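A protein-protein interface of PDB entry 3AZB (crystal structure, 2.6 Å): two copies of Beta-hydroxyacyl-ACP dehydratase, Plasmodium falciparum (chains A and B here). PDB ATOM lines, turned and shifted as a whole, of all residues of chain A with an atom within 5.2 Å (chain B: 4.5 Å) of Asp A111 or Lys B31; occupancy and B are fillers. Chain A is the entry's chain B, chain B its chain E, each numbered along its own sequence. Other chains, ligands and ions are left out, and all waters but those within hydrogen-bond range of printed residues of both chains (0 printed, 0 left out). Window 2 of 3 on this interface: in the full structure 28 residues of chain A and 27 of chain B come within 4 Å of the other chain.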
ATOM      1  N   LYS A  45      15.847  23.243  10.775  1.00  0.00           N
ATOM      2  CA  LYS A  45      16.526  24.070   9.783  1.00  0.00           C
ATOM      3  C   LYS A  45      15.443  24.499   8.799  1.00  0.00           C
ATOM      4  O   LYS A  45      14.810  23.656   8.125  1.00  0.00           O
ATOM      5  CB  LYS A  45      17.654  23.293   9.082  1.00  0.00           C
ATOM      6  CG  LYS A  45      18.480  24.094   8.055  1.00  0.00           C
ATOM      7  CD  LYS A  45      17.908  23.994   6.631  1.00  0.00           C
ATOM      8  CE  LYS A  45      18.499  25.058   5.660  1.00  0.00           C
ATOM      9  NZ  LYS A  45      18.423  26.457   6.187  1.00  0.00           N
ATOM     10  N   GLN A  46      15.204  25.807   8.750  1.00  0.00           N
ATOM     11  CA  GLN A  46      14.139  26.349   7.931  1.00  0.00           C
ATOM     12  C   GLN A  46      14.643  26.503   6.503  1.00  0.00           C
ATOM     13  O   GLN A  46      15.726  27.022   6.260  1.00  0.00           O
ATOM     14  CB  GLN A  46      13.607  27.653   8.538  1.00  0.00           C
ATOM     15  CG  GLN A  46      13.080  27.515   9.997  1.00  0.00           C
ATOM     16  CD  GLN A  46      11.692  26.840  10.107  1.00  0.00           C
ATOM     17  OE1 GLN A  46      11.183  26.243   9.158  1.00  0.00           O
ATOM     18  NE2 GLN A  46      11.074  26.966  11.268  1.00  0.00           N
ATOM     19  N   VAL A  47      13.860  26.003   5.560  1.00  0.00           N
ATOM     20  CA  VAL A  47      14.238  25.959   4.157  1.00  0.00           C
ATOM     21  C   VAL A  47      13.523  27.101   3.461  1.00  0.00           C
ATOM     22  O   VAL A  47      12.333  27.006   3.223  1.00  0.00           O
ATOM     23  CB  VAL A  47      13.819  24.598   3.498  1.00  0.00           C
ATOM     24  CG1 VAL A  47      14.543  24.364   2.175  1.00  0.00           C
ATOM     25  CG2 VAL A  47      14.094  23.436   4.426  1.00  0.00           C
ATOM     26  N   PRO A 106      11.989  14.933  -1.614  1.00  0.00           N
ATOM     27  CA  PRO A 106      12.543  16.263  -1.833  1.00  0.00           C
ATOM     28  C   PRO A 106      12.199  17.233  -0.699  1.00  0.00           C
ATOM     29  O   PRO A 106      11.021  17.366  -0.325  1.00  0.00           O
ATOM     30  CB  PRO A 106      11.858  16.704  -3.130  1.00  0.00           C
ATOM     31  CG  PRO A 106      11.702  15.443  -3.889  1.00  0.00           C
ATOM     32  CD  PRO A 106      11.334  14.419  -2.836  1.00  0.00           C
ATOM     33  N   VAL A 107      13.226  17.891  -0.155  1.00  0.00           N
ATOM     34  CA  VAL A 107      13.018  19.041   0.738  1.00  0.00           C
ATOM     35  C   VAL A 107      12.959  20.319  -0.116  1.00  0.00           C
ATOM     36  O   VAL A 107      13.874  20.617  -0.896  1.00  0.00           O
ATOM     37  CB  VAL A 107      14.111  19.148   1.822  1.00  0.00           C
ATOM     38  CG1 VAL A 107      13.794  20.276   2.794  1.00  0.00           C
ATOM     39  CG2 VAL A 107      14.226  17.856   2.595  1.00  0.00           C
ATOM     40  N   LEU A 108      11.870  21.065   0.022  1.00  0.00           N
ATOM     41  CA  LEU A 108      11.619  22.215  -0.857  1.00  0.00           C
ATOM     42  C   LEU A 108      11.557  23.513  -0.059  1.00  0.00           C
ATOM     43  O   LEU A 108      11.417  23.474   1.176  1.00  0.00           O
ATOM     44  CB  LEU A 108      10.309  22.018  -1.629  1.00  0.00           C
ATOM     45  CG  LEU A 108      10.134  20.739  -2.466  1.00  0.00           C
ATOM     46  CD1 LEU A 108       8.668  20.541  -2.809  1.00  0.00           C
ATOM     47  CD2 LEU A 108      10.985  20.756  -3.735  1.00  0.00           C
ATOM     48  N   PRO A 109      11.670  24.661  -0.757  1.00  0.00           N
ATOM     49  CA  PRO A 109      11.430  25.961  -0.145  1.00  0.00           C
ATOM     50  C   PRO A 109      10.068  25.976   0.525  1.00  0.00           C
ATOM     51  O   PRO A 109       9.098  25.576  -0.083  1.00  0.00           O
ATOM     52  CB  PRO A 109      11.429  26.913  -1.346  1.00  0.00           C
ATOM     53  CG  PRO A 109      12.304  26.259  -2.341  1.00  0.00           C
ATOM     54  CD  PRO A 109      12.154  24.785  -2.146  1.00  0.00           C
ATOM     55  N   GLY A 110      10.005  26.423   1.771  1.00  0.00           N
ATOM     56  CA  GLY A 110       8.749  26.455   2.519  1.00  0.00           C
ATOM     57  C   GLY A 110       8.668  25.463   3.676  1.00  0.00           C
ATOM     58  O   GLY A 110       7.938  25.687   4.642  1.00  0.00           O
ATOM     59  N   ASP A 111       9.415  24.368   3.576  1.00  0.00           N
ATOM     60  CA  ASP A 111       9.378  23.295   4.578  1.00  0.00           C
ATOM     61  C   ASP A 111      10.103  23.648   5.878  1.00  0.00           C
ATOM     62  O   ASP A 111      10.944  24.556   5.909  1.00  0.00           O
ATOM     63  CB  ASP A 111      10.028  22.041   4.011  1.00  0.00           C
ATOM     64  CG  ASP A 111       9.301  21.503   2.825  1.00  0.00           C
ATOM     65  OD1 ASP A 111       8.118  21.859   2.651  1.00  0.00           O
ATOM     66  OD2 ASP A 111       9.902  20.714   2.067  1.00  0.00           O
ATOM     67  N   THR A 112       9.767  22.925   6.942  1.00  0.00           N
ATOM     68  CA  THR A 112      10.567  22.931   8.151  1.00  0.00           C
ATOM     69  C   THR A 112      11.202  21.549   8.171  1.00  0.00           C
ATOM     70  O   THR A 112      10.487  20.537   8.188  1.00  0.00           O
ATOM     71  CB  THR A 112       9.732  23.106   9.450  1.00  0.00           C
ATOM     72  OG1 THR A 112       8.993  24.335   9.415  1.00  0.00           O
ATOM     73  CG2 THR A 112      10.636  23.087  10.673  1.00  0.00           C
ATOM     74  N   LEU A 113      12.535  21.513   8.122  1.00  0.00           N
ATOM     75  CA  LEU A 113      13.277  20.280   8.303  1.00  0.00           C
ATOM     76  C   LEU A 113      13.545  20.115   9.798  1.00  0.00           C
ATOM     77  O   LEU A 113      14.366  20.832  10.400  1.00  0.00           O
ATOM     78  CB  LEU A 113      14.574  20.287   7.481  1.00  0.00           C
ATOM     79  CG  LEU A 113      15.622  19.166   7.649  1.00  0.00           C
ATOM     80  CD1 LEU A 113      15.042  17.809   7.297  1.00  0.00           C
ATOM     81  CD2 LEU A 113      16.898  19.433   6.806  1.00  0.00           C
ATOM     82  N   VAL A 137       9.896  16.258   7.438  1.00  0.00           N
ATOM     83  CA  VAL A 137       9.100  17.405   7.020  1.00  0.00           C
ATOM     84  C   VAL A 137       7.624  17.033   7.140  1.00  0.00           C
ATOM     85  O   VAL A 137       7.137  16.146   6.428  1.00  0.00           O
ATOM     86  CB  VAL A 137       9.436  17.901   5.588  1.00  0.00           C
ATOM     87  CG1 VAL A 137       8.397  18.934   5.115  1.00  0.00           C
ATOM     88  CG2 VAL A 137      10.856  18.464   5.523  1.00  0.00           C
ATOM     89  N   SER B  10      -2.190  24.953  -3.553  1.00  0.00           N
ATOM     90  CA  SER B  10      -0.980  25.677  -3.201  1.00  0.00           C
ATOM     91  C   SER B  10      -0.143  26.015  -4.425  1.00  0.00           C
ATOM     92  O   SER B  10       0.138  25.152  -5.262  1.00  0.00           O
ATOM     93  CB  SER B  10      -0.133  24.903  -2.200  1.00  0.00           C
ATOM     94  OG  SER B  10       1.136  25.529  -2.065  1.00  0.00           O
ATOM     95  N   ILE B  11       0.242  27.286  -4.515  1.00  0.00           N
ATOM     96  CA  ILE B  11       1.219  27.731  -5.498  1.00  0.00           C
ATOM     97  C   ILE B  11       2.626  27.646  -4.886  1.00  0.00           C
ATOM     98  O   ILE B  11       3.023  28.495  -4.088  1.00  0.00           O
ATOM     99  CB  ILE B  11       0.926  29.167  -6.007  1.00  0.00           C
ATOM    100  CG1 ILE B  11      -0.543  29.298  -6.441  1.00  0.00           C
ATOM    101  CG2 ILE B  11       1.886  29.531  -7.146  1.00  0.00           C
ATOM    102  CD1 ILE B  11      -1.033  30.726  -6.573  1.00  0.00           C
ATOM    103  N   ILE B  16       5.459  30.694  -8.129  1.00  0.00           N
ATOM    104  CA  ILE B  16       5.681  32.052  -7.593  1.00  0.00           C
ATOM    105  C   ILE B  16       6.635  32.893  -8.471  1.00  0.00           C
ATOM    106  O   ILE B  16       6.373  34.085  -8.739  1.00  0.00           O
ATOM    107  CB  ILE B  16       6.206  32.014  -6.128  1.00  0.00           C
ATOM    108  CG1 ILE B  16       5.099  31.545  -5.169  1.00  0.00           C
ATOM    109  CG2 ILE B  16       6.752  33.381  -5.702  1.00  0.00           C
ATOM    110  CD1 ILE B  16       5.513  31.423  -3.726  1.00  0.00           C
ATOM    111  N   VAL B  29       9.138  35.295  -0.432  1.00  0.00           N
ATOM    112  CA  VAL B  29       7.909  34.508  -0.279  1.00  0.00           C
ATOM    113  C   VAL B  29       8.253  33.089  -0.662  1.00  0.00           C
ATOM    114  O   VAL B  29       8.579  32.816  -1.822  1.00  0.00           O
ATOM    115  CB  VAL B  29       6.767  35.018  -1.190  1.00  0.00           C
ATOM    116  CG1 VAL B  29       5.510  34.172  -1.005  1.00  0.00           C
ATOM    117  CG2 VAL B  29       6.453  36.483  -0.902  1.00  0.00           C
ATOM    118  N   ASP B  30       8.196  32.184   0.313  1.00  0.00           N
ATOM    119  CA  ASP B  30       8.594  30.801   0.088  1.00  0.00           C
ATOM    120  C   ASP B  30       7.480  29.921  -0.475  1.00  0.00           C
ATOM    121  O   ASP B  30       7.741  29.088  -1.339  1.00  0.00           O
ATOM    122  CB  ASP B  30       9.184  30.206   1.359  1.00  0.00           C
ATOM    123  CG  ASP B  30      10.588  30.706   1.630  1.00  0.00           C
ATOM    124  OD1 ASP B  30      11.335  30.947   0.677  1.00  0.00           O
ATOM    125  OD2 ASP B  30      10.966  30.848   2.798  1.00  0.00           O
ATOM    126  N   LYS B  31       6.254  30.117   0.023  1.00  0.00           N
ATOM    127  CA  LYS B  31       5.084  29.365  -0.414  1.00  0.00           C
ATOM    128  C   LYS B  31       3.791  30.168  -0.232  1.00  0.00           C
ATOM    129  O   LYS B  31       3.694  31.037   0.638  1.00  0.00           O
ATOM    130  CB  LYS B  31       4.999  28.023   0.335  1.00  0.00           C
ATOM    131  CG  LYS B  31       4.115  26.948  -0.336  1.00  0.00           C
ATOM    132  CD  LYS B  31       3.905  25.751   0.577  1.00  0.00           C
ATOM    133  CE  LYS B  31       4.960  24.662   0.371  1.00  0.00           C
ATOM    134  NZ  LYS B  31       4.831  23.545   1.376  1.00  0.00           N
ATOM    135  N   VAL B  32       2.805  29.880  -1.075  1.00  0.00           N
ATOM    136  CA  VAL B  32       1.468  30.439  -0.929  1.00  0.00           C
ATOM    137  C   VAL B  32       0.521  29.286  -0.592  1.00  0.00           C
ATOM    138  O   VAL B  32       0.413  28.315  -1.345  1.00  0.00           O
ATOM    139  CB  VAL B  32       1.023  31.205  -2.197  1.00  0.00           C
ATOM    140  CG1 VAL B  32      -0.455  31.584  -2.119  1.00  0.00           C
ATOM    141  CG2 VAL B  32       1.883  32.466  -2.387  1.00  0.00           C
ATOM    142  N   ILE B  33      -0.133  29.372   0.562  1.00  0.00           N
ATOM    143  CA  ILE B  33      -0.910  28.235   1.064  1.00  0.00           C
ATOM    144  C   ILE B  33      -2.392  28.400   0.731  1.00  0.00           C
ATOM    145  O   ILE B  33      -3.075  27.425   0.401  1.00  0.00           O
ATOM    146  CB  ILE B  33      -0.658  27.940   2.572  1.00  0.00           C
ATOM    147  CG1 ILE B  33      -0.806  29.207   3.431  1.00  0.00           C
ATOM    148  CG2 ILE B  33       0.738  27.337   2.762  1.00  0.00           C
ATOM    149  CD1 ILE B  33      -0.933  28.956   4.922  1.00  0.00           C
ATOM    150  N   ILE B  42      -2.671  34.135   1.700  1.00  0.00           N
ATOM    151  CA  ILE B  42      -1.814  33.715   2.798  1.00  0.00           C
ATOM    152  C   ILE B  42      -0.542  33.026   2.282  1.00  0.00           C
ATOM    153  O   ILE B  42      -0.575  32.117   1.436  1.00  0.00           O
ATOM    154  CB  ILE B  42      -2.564  32.851   3.834  1.00  0.00           C
ATOM    155  CG1 ILE B  42      -3.862  33.554   4.258  1.00  0.00           C
ATOM    156  CG2 ILE B  42      -1.679  32.582   5.047  1.00  0.00           C
ATOM    157  CD1 ILE B  42      -4.852  32.656   4.998  1.00  0.00           C
ATOM    158  N   GLY B  43       0.586  33.493   2.789  1.00  0.00           N
ATOM    159  CA  GLY B  43       1.864  32.918   2.426  1.00  0.00           C
ATOM    160  C   GLY B  43       2.731  32.697   3.641  1.00  0.00           C
ATOM    161  O   GLY B  43       2.383  33.076   4.762  1.00  0.00           O
ATOM    162  N   LEU B  44       3.868  32.071   3.415  1.00  0.00           N
ATOM    163  CA  LEU B  44       4.866  31.949   4.460  1.00  0.00           C
ATOM    164  C   LEU B  44       6.260  32.251   3.914  1.00  0.00           C
ATOM    165  O   LEU B  44       6.499  32.162   2.706  1.00  0.00           O
ATOM    166  CB  LEU B  44       4.787  30.575   5.155  1.00  0.00           C
ATOM    167  CG  LEU B  44       4.718  29.292   4.318  1.00  0.00           C
ATOM    168  CD1 LEU B  44       6.118  28.873   3.890  1.00  0.00           C
ATOM    169  CD2 LEU B  44       4.014  28.129   5.065  1.00  0.00           C
ATOM    170  N   GLN B  46      10.136  31.107   5.312  1.00  0.00           N
ATOM    171  CA  GLN B  46      10.946  30.404   6.289  1.00  0.00           C
ATOM    172  C   GLN B  46      12.216  31.208   6.559  1.00  0.00           C
ATOM    173  O   GLN B  46      12.980  31.499   5.634  1.00  0.00           O
ATOM    174  CB  GLN B  46      11.310  29.009   5.787  1.00  0.00           C
ATOM    175  CG  GLN B  46      10.147  28.096   5.567  1.00  0.00           C
ATOM    176  CD  GLN B  46       9.527  27.571   6.861  1.00  0.00           C
ATOM    177  OE1 GLN B  46       9.827  28.039   7.959  1.00  0.00           O
ATOM    178  NE2 GLN B  46       8.643  26.600   6.728  1.00  0.00           N
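OD1 of Asp A111 lies within salt-bridge range of NZ of Lys B31, 3.9 Å away. The side-chain amide oxygen (OE1) of Gln A46 lies close to the side-chain amide oxygen (OE1) of Gln B46 (2.5 Å). O of Asp A111 lies within hydrogen-bond range of NE2 of Gln B46. The backbone carbonyl oxygen (O) of Gly A110 lies close to the side-chain amide nitrogen (NE2) of Gln B46, at 2.4 Å.
The side-chain carboxylate of Asp B30 lies within hydrogen-bond range of the backbone NH of Gln B46, 2.7 Å away. The backbone NH (N) of Leu B44 is in hydrogen-bond range of the backbone carbonyl oxygen (O) of Lys B31, 3.0 Å away. The backbone carbonyl oxygen (O) of Val A47 lies within hydrogen-bond range of the backbone NH (N) of Gly A110 (2.8 Å). N of Asp B30 sits at hydrogen-bond distance from O of Leu B44. OG1 of Thr A112 is in hydrogen-bond range of OE1 of Gln A46, 2.9 Å away. The backbone carbonyl oxygen (O) of Asp A111 is in hydrogen-bond range of the backbone NH (N) of Val A47, at 3.3 Å.
Among the printed residues, merely in contact across the chains: Val A47 with Gln B46, Thr A112 with Gln B46, Gly A110 with Leu B44, Gly A110 with Asp B30 and Pro A109 with Asp B30.
Asp A111 touches just these residues of chain B: Lys B31 and Gln B46. Lys B31 touches just one residue of chain A: Asp A111. Of the printed residues of chain B, Gln A46 touches Gln B46. Printed residues of chain B within 4 Å of Pro A109: Asp B30. Printed residues of chain B within 4 Å of Thr A112: Gln B46 (3.5 Å). Printed residues of chain A within 4 Å of Leu B44: Gly A110. Ile B16 touches none of the printed residues of chain A. The nearest printed residue of chain B that does not touch Gln A46 is Asp B30 (6.8 Å).
Hydrophobic or aromatic side chains of chain B within 4 Å of the printed part of chain A: Leu B44. Among the printed residues, 9 pairs touch across the chains.
Gln B46 touches its own counterpart, Gln A46. 1 position is printed for both chains. Of the 9 pairs that touch across the chains among the printed residues, 1 has its exchanged pair printed and touching as well.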
